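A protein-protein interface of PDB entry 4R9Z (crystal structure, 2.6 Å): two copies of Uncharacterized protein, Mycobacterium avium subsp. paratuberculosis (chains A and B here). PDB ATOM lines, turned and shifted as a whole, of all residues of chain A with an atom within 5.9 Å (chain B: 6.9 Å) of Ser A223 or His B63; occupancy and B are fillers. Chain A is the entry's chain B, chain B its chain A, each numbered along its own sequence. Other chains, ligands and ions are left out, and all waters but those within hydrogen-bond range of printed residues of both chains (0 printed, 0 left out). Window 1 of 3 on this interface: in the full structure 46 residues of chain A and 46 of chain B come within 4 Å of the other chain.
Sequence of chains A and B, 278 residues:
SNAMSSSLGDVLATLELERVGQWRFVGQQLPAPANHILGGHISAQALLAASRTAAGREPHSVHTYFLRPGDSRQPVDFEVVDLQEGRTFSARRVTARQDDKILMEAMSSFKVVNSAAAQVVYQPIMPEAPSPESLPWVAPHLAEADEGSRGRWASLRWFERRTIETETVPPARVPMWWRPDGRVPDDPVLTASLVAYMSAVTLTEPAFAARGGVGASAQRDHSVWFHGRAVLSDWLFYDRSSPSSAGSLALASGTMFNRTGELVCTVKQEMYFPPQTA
Of the 16 printed residues of chain B, 11 touch a printed residue of chain A. Hydrophobic or aromatic side chains of chain B within 4 Å of the printed part of chain A: His B63, Tyr B65, Met B107 and Trp B225. Hydrophobic or aromatic side chains of chain A that line the printed part of chain B: His A63, Tyr A65, Met A107 and Trp A225. Among the printed residues, 23 pairs touch across the chains.
OG of Ser B61 sits at hydrogen-bond distance from OH of Tyr A65 (2.6 Å). A ring nitrogen (ND1) of His B63 is in hydrogen-bond range of a ring nitrogen (ND1) of His A63, at 3.2 Å. A ring nitrogen (NE2) of His B63 lies within hydrogen-bond range of the side-chain carboxylate (OD2) of Asp A221, 3.1 Å away. ND1 of His B63 sits close to OG of Ser A223. The side-chain carboxylate (OD1) of Asp B221 lies within hydrogen-bond range of the indole nitrogen (NE1) of Trp A225. ND1 of His A63 sits close to OG of Ser B223 (3.5 Å). NE1 of Trp B225 lies within hydrogen-bond range of OD2 of Asp A221. O of Glu B105 sits close to SD of Met A107 (3.7 Å).
His B63 touches just these residues of chain A: His A63, Tyr A65, Met A107, Asp A221 and Ser A223. Of the printed residues of chain A, Tyr B65 touches Val A62, His A63 and Met A107. Of the printed residues of chain A, Ser B109 touches Tyr A65. Of the printed residues of chain A, Ser B223 touches His A63 (3.2 Å). Of the printed residues of chain A, Trp B225 touches Asp A221 (3.0 Å), Trp A225 (3.9 Å) and Lys A268 (3.5 Å). The nearest residue of chain B that does not touch Ser A223 is Trp B225 (4.1 Å).
N of His B63 lies within hydrogen-bond range of O of Met B107 (2.8 Å). ND1 of His B63 sits at hydrogen-bond distance from OG of Ser B223 (2.6 Å). The backbone carbonyl oxygen (O) of Met A107 is in hydrogen-bond range of the backbone NH (N) of His A63 (2.7 Å). A ring nitrogen (ND1) of His A63 lies within hydrogen-bond range of the side-chain hydroxyl (OG) of Ser A223 (2.8 Å). The backbone NH (N) of Ser A223 is in hydrogen-bond range of the backbone carbonyl oxygen (O) of Lys A268 (2.8 Å). The backbone NH (N) of Trp A225 lies within hydrogen-bond range of the backbone carbonyl oxygen (O) of Thr A266 (2.8 Å).
Val A62 touches Tyr B65, and with the chains exchanged Tyr A65 touches Val B62. His B63 touches its own counterpart, His A63. His A63 touches Tyr B65, and with the chains exchanged Tyr A65 touches His B63. Met B107 touches its own counterpart, Met A107. 10 positions are printed for both chains. Of the 23 pairs that touch across the chains among the printed residues, 17 have their exchanged pair printed and touching as well.
Among the printed residues, pairs that only touch across the chains: Val A62 with Tyr B65 (3.5 Å), His A63 with Tyr B65 (3.3 Å), His A63 with Met B107 (3.4 Å), His A63 with Asp B221 (3.6 Å), Tyr A65 with Val B62 (3.7 Å), Tyr A65 with His B63 (3.5 Å), Tyr A65 with Met B107 (3.5 Å), Tyr A65 with Ser B108 (3.8 Å), Tyr A65 with Ser B109 (3.5 Å), Met A107 with His B63 (3.3 Å), Met A107 with Tyr B65 (3.5 Å), Met A107 with Met B107 (3.9 Å), Asp A221 with Ser B61 (3.8 Å), Trp A225 with Trp B225 (3.9 Å) and Lys A268 with Trp B225 (3.5 Å).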
ATOM      1  N   VAL A  62      11.998 -15.631   2.925  1.00  0.00           N
ATOM      2  CA  VAL A  62      12.677 -16.814   3.433  1.00  0.00           C
ATOM      3  C   VAL A  62      14.114 -16.867   2.904  1.00  0.00           C
ATOM      4  O   VAL A  62      14.376 -16.598   1.731  1.00  0.00           O
ATOM      5  CB  VAL A  62      11.916 -18.122   3.049  1.00  0.00           C
ATOM      6  CG1 VAL A  62      11.694 -18.209   1.548  1.00  0.00           C
ATOM      7  CG2 VAL A  62      12.658 -19.356   3.550  1.00  0.00           C
ATOM      8  N   HIS A  63      15.046 -17.205   3.784  1.00  0.00           N
ATOM      9  CA  HIS A  63      16.449 -17.296   3.419  1.00  0.00           C
ATOM     10  C   HIS A  63      16.965 -18.674   3.775  1.00  0.00           C
ATOM     11  O   HIS A  63      16.879 -19.090   4.925  1.00  0.00           O
ATOM     12  CB  HIS A  63      17.252 -16.209   4.129  1.00  0.00           C
ATOM     13  CG  HIS A  63      16.753 -14.826   3.854  1.00  0.00           C
ATOM     14  ND1 HIS A  63      17.173 -14.085   2.773  1.00  0.00           N
ATOM     15  CD2 HIS A  63      15.849 -14.058   4.508  1.00  0.00           C
ATOM     16  CE1 HIS A  63      16.559 -12.915   2.777  1.00  0.00           C
ATOM     17  NE2 HIS A  63      15.751 -12.874   3.821  1.00  0.00           N
ATOM     18  N   THR A  64      17.495 -19.385   2.785  1.00  0.00           N
ATOM     19  CA  THR A  64      17.896 -20.768   2.986  1.00  0.00           C
ATOM     20  C   THR A  64      19.355 -20.996   2.606  1.00  0.00           C
ATOM     21  O   THR A  64      19.775 -20.621   1.518  1.00  0.00           O
ATOM     22  CB  THR A  64      17.011 -21.716   2.159  1.00  0.00           C
ATOM     23  OG1 THR A  64      15.627 -21.403   2.372  1.00  0.00           O
ATOM     24  CG2 THR A  64      17.271 -23.154   2.541  1.00  0.00           C
ATOM     25  N   TYR A  65      20.122 -21.612   3.504  1.00  0.00           N
ATOM     26  CA  TYR A  65      21.482 -22.042   3.189  1.00  0.00           C
ATOM     27  C   TYR A  65      21.513 -23.538   2.952  1.00  0.00           C
ATOM     28  O   TYR A  65      21.036 -24.298   3.778  1.00  0.00           O
ATOM     29  CB  TYR A  65      22.462 -21.694   4.320  1.00  0.00           C
ATOM     30  CG  TYR A  65      23.164 -20.372   4.137  1.00  0.00           C
ATOM     31  CD1 TYR A  65      24.047 -20.176   3.088  1.00  0.00           C
ATOM     32  CD2 TYR A  65      22.939 -19.320   5.007  1.00  0.00           C
ATOM     33  CE1 TYR A  65      24.680 -18.967   2.911  1.00  0.00           C
ATOM     34  CE2 TYR A  65      23.571 -18.107   4.838  1.00  0.00           C
ATOM     35  CZ  TYR A  65      24.441 -17.935   3.791  1.00  0.00           C
ATOM     36  OH  TYR A  65      25.070 -16.728   3.623  1.00  0.00           O
ATOM     37  N   MET A 107      15.854 -19.248   7.492  1.00  0.00           N
ATOM     38  CA  MET A 107      15.049 -18.323   8.268  1.00  0.00           C
ATOM     39  C   MET A 107      13.888 -17.848   7.419  1.00  0.00           C
ATOM     40  O   MET A 107      14.008 -17.737   6.207  1.00  0.00           O
ATOM     41  CB  MET A 107      15.878 -17.146   8.767  1.00  0.00           C
ATOM     42  CG  MET A 107      17.014 -17.543   9.686  1.00  0.00           C
ATOM     43  SD  MET A 107      17.864 -16.105  10.347  1.00  0.00           S
ATOM     44  CE  MET A 107      18.532 -15.408   8.848  1.00  0.00           C
ATOM     45  N   ASP A 221      22.991 -20.906  -1.339  1.00  0.00           N
ATOM     46  CA  ASP A 221      21.849 -20.311  -0.662  1.00  0.00           C
ATOM     47  C   ASP A 221      20.766 -19.829  -1.624  1.00  0.00           C
ATOM     48  O   ASP A 221      21.013 -19.605  -2.806  1.00  0.00           O
ATOM     49  CB  ASP A 221      22.300 -19.171   0.273  1.00  0.00           C
ATOM     50  CG  ASP A 221      23.118 -18.097  -0.426  1.00  0.00           C
ATOM     51  OD1 ASP A 221      24.328 -18.321  -0.655  1.00  0.00           O
ATOM     52  OD2 ASP A 221      22.566 -17.011  -0.700  1.00  0.00           O
ATOM     53  N   HIS A 222      19.555 -19.701  -1.089  1.00  0.00           N
ATOM     54  CA  HIS A 222      18.387 -19.284  -1.851  1.00  0.00           C
ATOM     55  C   HIS A 222      17.568 -18.302  -1.026  1.00  0.00           C
ATOM     56  O   HIS A 222      17.305 -18.541   0.150  1.00  0.00           O
ATOM     57  CB  HIS A 222      17.534 -20.495  -2.227  1.00  0.00           C
ATOM     58  CG  HIS A 222      16.384 -20.175  -3.129  1.00  0.00           C
ATOM     59  ND1 HIS A 222      16.547 -19.878  -4.466  1.00  0.00           N
ATOM     60  CD2 HIS A 222      15.054 -20.098  -2.885  1.00  0.00           C
ATOM     61  CE1 HIS A 222      15.368 -19.641  -5.008  1.00  0.00           C
ATOM     62  NE2 HIS A 222      14.444 -19.769  -4.071  1.00  0.00           N
ATOM     63  N   SER A 223      17.137 -17.219  -1.655  1.00  0.00           N
ATOM     64  CA  SER A 223      16.391 -16.175  -0.968  1.00  0.00           C
ATOM     65  C   SER A 223      15.168 -15.790  -1.781  1.00  0.00           C
ATOM     66  O   SER A 223      15.271 -15.586  -2.992  1.00  0.00           O
ATOM     67  CB  SER A 223      17.262 -14.935  -0.746  1.00  0.00           C
ATOM     68  OG  SER A 223      18.162 -15.094   0.332  1.00  0.00           O
ATOM     69  N   VAL A 224      14.009 -15.725  -1.126  1.00  0.00           N
ATOM     70  CA  VAL A 224      12.770 -15.338  -1.800  1.00  0.00           C
ATOM     71  C   VAL A 224      12.020 -14.268  -1.018  1.00  0.00           C
ATOM     72  O   VAL A 224      11.793 -14.414   0.177  1.00  0.00           O
ATOM     73  CB  VAL A 224      11.830 -16.530  -2.004  1.00  0.00           C
ATOM     74  CG1 VAL A 224      10.607 -16.100  -2.793  1.00  0.00           C
ATOM     75  CG2 VAL A 224      12.543 -17.651  -2.715  1.00  0.00           C
ATOM     76  N   TRP A 225      11.605 -13.210  -1.703  1.00  0.00           N
ATOM     77  CA  TRP A 225      10.728 -12.216  -1.104  1.00  0.00           C
ATOM     78  C   TRP A 225       9.383 -12.238  -1.819  1.00  0.00           C
ATOM     79  O   TRP A 225       9.304 -12.011  -3.027  1.00  0.00           O
ATOM     80  CB  TRP A 225      11.360 -10.821  -1.176  1.00  0.00           C
ATOM     81  CG  TRP A 225      12.674 -10.727  -0.469  1.00  0.00           C
ATOM     82  CD1 TRP A 225      12.889 -10.299   0.809  1.00  0.00           C
ATOM     83  CD2 TRP A 225      13.958 -11.087  -0.993  1.00  0.00           C
ATOM     84  NE1 TRP A 225      14.229 -10.361   1.110  1.00  0.00           N
ATOM     85  CE2 TRP A 225      14.905 -10.842   0.020  1.00  0.00           C
ATOM     86  CE3 TRP A 225      14.399 -11.587  -2.222  1.00  0.00           C
ATOM     87  CZ2 TRP A 225      16.261 -11.079  -0.157  1.00  0.00           C
ATOM     88  CZ3 TRP A 225      15.747 -11.821  -2.394  1.00  0.00           C
ATOM     89  CH2 TRP A 225      16.663 -11.567  -1.365  1.00  0.00           C
ATOM     90  N   THR A 266      10.368 -11.933  -5.643  1.00  0.00           N
ATOM     91  CA  THR A 266      11.711 -11.556  -6.071  1.00  0.00           C
ATOM     92  C   THR A 266      12.662 -12.592  -5.494  1.00  0.00           C
ATOM     93  O   THR A 266      12.467 -13.047  -4.371  1.00  0.00           O
ATOM     94  CB  THR A 266      12.103 -10.144  -5.591  1.00  0.00           C
ATOM     95  OG1 THR A 266      11.094  -9.203  -5.974  1.00  0.00           O
ATOM     96  CG2 THR A 266      13.432  -9.723  -6.191  1.00  0.00           C
ATOM     97  N   VAL A 267      13.687 -12.973  -6.252  1.00  0.00           N
ATOM     98  CA  VAL A 267      14.512 -14.127  -5.895  1.00  0.00           C
ATOM     99  C   VAL A 267      16.002 -13.869  -6.107  1.00  0.00           C
ATOM    100  O   VAL A 267      16.394 -13.210  -7.071  1.00  0.00           O
ATOM    101  CB  VAL A 267      14.114 -15.377  -6.720  1.00  0.00           C
ATOM    102  CG1 VAL A 267      14.886 -16.594  -6.258  1.00  0.00           C
ATOM    103  CG2 VAL A 267      12.627 -15.647  -6.611  1.00  0.00           C
ATOM    104  N   LYS A 268      16.830 -14.381  -5.199  1.00  0.00           N
ATOM    105  CA  LYS A 268      18.278 -14.359  -5.377  1.00  0.00           C
ATOM    106  C   LYS A 268      18.884 -15.696  -4.966  1.00  0.00           C
ATOM    107  O   LYS A 268      18.468 -16.291  -3.977  1.00  0.00           O
ATOM    108  CB  LYS A 268      18.913 -13.229  -4.570  1.00  0.00           C
ATOM    109  CG  LYS A 268      20.323 -12.879  -5.019  1.00  0.00           C
ATOM    110  CD  LYS A 268      20.307 -12.023  -6.273  1.00  0.00           C
ATOM    111  CE  LYS A 268      19.930 -10.587  -5.956  1.00  0.00           C
ATOM    112  NZ  LYS A 268      19.848  -9.756  -7.191  1.00  0.00           N
ATOM    113  N   GLN A 269      19.874 -16.163  -5.720  1.00  0.00           N
ATOM    114  CA  GLN A 269      20.492 -17.451  -5.435  1.00  0.00           C
ATOM    115  C   GLN A 269      21.999 -17.422  -5.658  1.00  0.00           C
ATOM    116  O   GLN A 269      22.485 -16.912  -6.667  1.00  0.00           O
ATOM    117  CB  GLN A 269      19.864 -18.547  -6.299  1.00  0.00           C
ATOM    118  CG  GLN A 269      20.422 -19.939  -6.033  1.00  0.00           C
ATOM    119  CD  GLN A 269      19.794 -20.998  -6.913  1.00  0.00           C
ATOM    120  OE1 GLN A 269      20.492 -21.738  -7.605  1.00  0.00           O
ATOM    121  NE2 GLN A 269      18.468 -21.073  -6.897  1.00  0.00           N
ATOM    122  N   SER B  61      28.721 -14.235   1.850  1.00  0.00           N
ATOM    123  CA  SER B  61      27.330 -13.797   1.974  1.00  0.00           C
ATOM    124  C   SER B  61      26.841 -13.800   3.420  1.00  0.00           C
ATOM    125  O   SER B  61      27.431 -14.431   4.299  1.00  0.00           O
ATOM    126  CB  SER B  61      26.385 -14.655   1.112  1.00  0.00           C
ATOM    127  OG  SER B  61      26.352 -16.008   1.523  1.00  0.00           O
ATOM    128  N   VAL B  62      25.751 -13.079   3.650  1.00  0.00           N
ATOM    129  CA  VAL B  62      25.151 -12.983   4.967  1.00  0.00           C
ATOM    130  C   VAL B  62      23.683 -12.566   4.847  1.00  0.00           C
ATOM    131  O   VAL B  62      23.335 -11.694   4.053  1.00  0.00           O
ATOM    132  CB  VAL B  62      25.942 -11.987   5.872  1.00  0.00           C
ATOM    133  CG1 VAL B  62      26.152 -10.659   5.174  1.00  0.00           C
ATOM    134  CG2 VAL B  62      25.264 -11.807   7.227  1.00  0.00           C
ATOM    135  N   HIS B  63      22.829 -13.227   5.621  1.00  0.00           N
ATOM    136  CA  HIS B  63      21.401 -12.936   5.648  1.00  0.00           C
ATOM    137  C   HIS B  63      20.961 -12.641   7.072  1.00  0.00           C
ATOM    138  O   HIS B  63      21.103 -13.484   7.953  1.00  0.00           O
ATOM    139  CB  HIS B  63      20.585 -14.109   5.106  1.00  0.00           C
ATOM    140  CG  HIS B  63      20.953 -14.515   3.717  1.00  0.00           C
ATOM    141  ND1 HIS B  63      20.387 -13.939   2.601  1.00  0.00           N
ATOM    142  CD2 HIS B  63      21.829 -15.442   3.261  1.00  0.00           C
ATOM    143  CE1 HIS B  63      20.901 -14.491   1.516  1.00  0.00           C
ATOM    144  NE2 HIS B  63      21.778 -15.404   1.889  1.00  0.00           N
ATOM    145  N   THR B  64      20.395 -11.464   7.293  1.00  0.00           N
ATOM    146  CA  THR B  64      20.045 -11.048   8.641  1.00  0.00           C
ATOM    147  C   THR B  64      18.577 -10.692   8.744  1.00  0.00           C
ATOM    148  O   THR B  64      18.065  -9.966   7.903  1.00  0.00           O
ATOM    149  CB  THR B  64      20.860  -9.826   9.099  1.00  0.00           C
ATOM    150  OG1 THR B  64      22.255 -10.050   8.870  1.00  0.00           O
ATOM    151  CG2 THR B  64      20.627  -9.560  10.578  1.00  0.00           C
ATOM    152  N   TYR B  65      17.900 -11.223   9.758  1.00  0.00           N
ATOM    153  CA  TYR B  65      16.542 -10.789  10.085  1.00  0.00           C
ATOM    154  C   TYR B  65      16.569  -9.872  11.297  1.00  0.00           C
ATOM    155  O   TYR B  65      17.188 -10.198  12.301  1.00  0.00           O
ATOM    156  CB  TYR B  65      15.636 -11.981  10.372  1.00  0.00           C
ATOM    157  CG  TYR B  65      14.883 -12.482   9.169  1.00  0.00           C
ATOM    158  CD1 TYR B  65      13.923 -11.694   8.541  1.00  0.00           C
ATOM    159  CD2 TYR B  65      15.123 -13.746   8.665  1.00  0.00           C
ATOM    160  CE1 TYR B  65      13.236 -12.155   7.436  1.00  0.00           C
ATOM    161  CE2 TYR B  65      14.440 -14.216   7.566  1.00  0.00           C
ATOM    162  CZ  TYR B  65      13.498 -13.420   6.955  1.00  0.00           C
ATOM    163  OH  TYR B  65      12.821 -13.899   5.860  1.00  0.00           O
ATOM    164  N   MET B 104      17.967  -9.936  16.673  1.00  0.00           N
ATOM    165  CA  MET B 104      18.179 -10.342  15.296  1.00  0.00           C
ATOM    166  C   MET B 104      18.784 -11.730  15.239  1.00  0.00           C
ATOM    167  O   MET B 104      19.396 -12.201  16.198  1.00  0.00           O
ATOM    168  CB  MET B 104      19.083  -9.343  14.551  1.00  0.00           C
ATOM    169  CG  MET B 104      20.446  -9.095  15.176  1.00  0.00           C
ATOM    170  SD  MET B 104      21.827  -9.317  14.025  1.00  0.00           S
ATOM    171  CE  MET B 104      21.983 -11.097  14.080  1.00  0.00           C
ATOM    172  N   GLU B 105      18.580 -12.397  14.112  1.00  0.00           N
ATOM    173  CA  GLU B 105      19.312 -13.614  13.830  1.00  0.00           C
ATOM    174  C   GLU B 105      19.916 -13.500  12.448  1.00  0.00           C
ATOM    175  O   GLU B 105      19.322 -12.903  11.551  1.00  0.00           O
ATOM    176  CB  GLU B 105      18.422 -14.849  13.928  1.00  0.00           C
ATOM    177  CG  GLU B 105      19.213 -16.131  13.785  1.00  0.00           C
ATOM    178  CD  GLU B 105      18.650 -17.263  14.609  1.00  0.00           C
ATOM    179  OE1 GLU B 105      18.843 -17.233  15.842  1.00  0.00           O
ATOM    180  OE2 GLU B 105      18.033 -18.184  14.028  1.00  0.00           O
ATOM    181  N   ALA B 106      21.104 -14.060  12.280  1.00  0.00           N
ATOM    182  CA  ALA B 106      21.785 -13.990  11.001  1.00  0.00           C
ATOM    183  C   ALA B 106      22.429 -15.321  10.663  1.00  0.00           C
ATOM    184  O   ALA B 106      22.835 -16.074  11.549  1.00  0.00           O
ATOM    185  CB  ALA B 106      22.818 -12.898  11.012  1.00  0.00           C
ATOM    186  N   MET B 107      22.474 -15.621   9.372  1.00  0.00           N
ATOM    187  CA  MET B 107      23.271 -16.722   8.862  1.00  0.00           C
ATOM    188  C   MET B 107      24.311 -16.146   7.927  1.00  0.00           C
ATOM    189  O   MET B 107      24.054 -15.179   7.210  1.00  0.00           O
ATOM    190  CB  MET B 107      22.412 -17.741   8.127  1.00  0.00           C
ATOM    191  CG  MET B 107      21.359 -18.397   8.972  1.00  0.00           C
ATOM    192  SD  MET B 107      20.478 -19.648   8.021  1.00  0.00           S
ATOM    193  CE  MET B 107      19.672 -18.635   6.787  1.00  0.00           C
ATOM    194  N   SER B 108      25.488 -16.744   7.925  1.00  0.00           N
ATOM    195  CA  SER B 108      26.566 -16.242   7.094  1.00  0.00           C
ATOM    196  C   SER B 108      27.390 -17.411   6.601  1.00  0.00           C
ATOM    197  O   SER B 108      27.435 -18.466   7.231  1.00  0.00           O
ATOM    198  CB  SER B 108      27.435 -15.251   7.864  1.00  0.00           C
ATOM    199  OG  SER B 108      27.868 -15.811   9.087  1.00  0.00           O
ATOM    200  N   SER B 109      28.051 -17.212   5.471  1.00  0.00           N
ATOM    201  CA  SER B 109      28.804 -18.274   4.839  1.00  0.00           C
ATOM    202  C   SER B 109      30.201 -17.765   4.505  1.00  0.00           C
ATOM    203  O   SER B 109      30.378 -16.591   4.176  1.00  0.00           O
ATOM    204  CB  SER B 109      28.063 -18.759   3.586  1.00  0.00           C
ATOM    205  OG  SER B 109      28.676 -19.890   2.995  1.00  0.00           O
ATOM    206  N   ASP B 221      14.727  -7.362   7.059  1.00  0.00           N
ATOM    207  CA  ASP B 221      15.884  -8.214   6.809  1.00  0.00           C
ATOM    208  C   ASP B 221      16.894  -7.548   5.889  1.00  0.00           C
ATOM    209  O   ASP B 221      16.578  -6.595   5.181  1.00  0.00           O
ATOM    210  CB  ASP B 221      15.477  -9.586   6.232  1.00  0.00           C
ATOM    211  CG  ASP B 221      14.696  -9.491   4.928  1.00  0.00           C
ATOM    212  OD1 ASP B 221      15.172  -8.819   3.986  1.00  0.00           O
ATOM    213  OD2 ASP B 221      13.619 -10.122   4.834  1.00  0.00           O
ATOM    214  N   HIS B 222      18.119  -8.057   5.928  1.00  0.00           N
ATOM    215  CA  HIS B 222      19.201  -7.526   5.118  1.00  0.00           C
ATOM    216  C   HIS B 222      20.010  -8.687   4.544  1.00  0.00           C
ATOM    217  O   HIS B 222      20.305  -9.651   5.250  1.00  0.00           O
ATOM    218  CB  HIS B 222      20.078  -6.595   5.959  1.00  0.00           C
ATOM    219  CG  HIS B 222      21.141  -5.890   5.177  1.00  0.00           C
ATOM    220  ND1 HIS B 222      20.859  -4.871   4.291  1.00  0.00           N
ATOM    221  CD2 HIS B 222      22.485  -6.041   5.161  1.00  0.00           C
ATOM    222  CE1 HIS B 222      21.984  -4.437   3.754  1.00  0.00           C
ATOM    223  NE2 HIS B 222      22.987  -5.128   4.266  1.00  0.00           N
ATOM    224  N   SER B 223      20.340  -8.612   3.260  1.00  0.00           N
ATOM    225  CA  SER B 223      21.093  -9.677   2.606  1.00  0.00           C
ATOM    226  C   SER B 223      22.215  -9.114   1.753  1.00  0.00           C
ATOM    227  O   SER B 223      22.012  -8.212   0.942  1.00  0.00           O
ATOM    228  CB  SER B 223      20.180 -10.551   1.747  1.00  0.00           C
ATOM    229  OG  SER B 223      19.453 -11.462   2.549  1.00  0.00           O
ATOM    230  N   VAL B 224      23.402  -9.675   1.933  1.00  0.00           N
ATOM    231  CA  VAL B 224      24.574  -9.218   1.213  1.00  0.00           C
ATOM    232  C   VAL B 224      25.285 -10.383   0.567  1.00  0.00           C
ATOM    233  O   VAL B 224      25.520 -11.398   1.207  1.00  0.00           O
ATOM    234  CB  VAL B 224      25.565  -8.505   2.146  1.00  0.00           C
ATOM    235  CG1 VAL B 224      26.743  -7.970   1.358  1.00  0.00           C
ATOM    236  CG2 VAL B 224      24.874  -7.393   2.912  1.00  0.00           C
ATOM    237  N   TRP B 225      25.618 -10.242  -0.706  1.00  0.00           N
ATOM    238  CA  TRP B 225      26.487 -11.208  -1.351  1.00  0.00           C
ATOM    239  C   TRP B 225      27.766 -10.492  -1.761  1.00  0.00           C
ATOM    240  O   TRP B 225      27.726  -9.512  -2.504  1.00  0.00           O
ATOM    241  CB  TRP B 225      25.801 -11.849  -2.556  1.00  0.00           C
ATOM    242  CG  TRP B 225      24.529 -12.561  -2.208  1.00  0.00           C
ATOM    243  CD1 TRP B 225      24.382 -13.889  -1.927  1.00  0.00           C
ATOM    244  CD2 TRP B 225      23.218 -11.983  -2.111  1.00  0.00           C
ATOM    245  NE1 TRP B 225      23.062 -14.173  -1.660  1.00  0.00           N
ATOM    246  CE2 TRP B 225      22.328 -13.020  -1.766  1.00  0.00           C
ATOM    247  CE3 TRP B 225      22.712 -10.692  -2.286  1.00  0.00           C
ATOM    248  CZ2 TRP B 225      20.959 -12.804  -1.592  1.00  0.00           C
ATOM    249  CZ3 TRP B 225      21.352 -10.479  -2.109  1.00  0.00           C
ATOM    250  CH2 TRP B 225      20.493 -11.529  -1.765  1.00  0.00           C
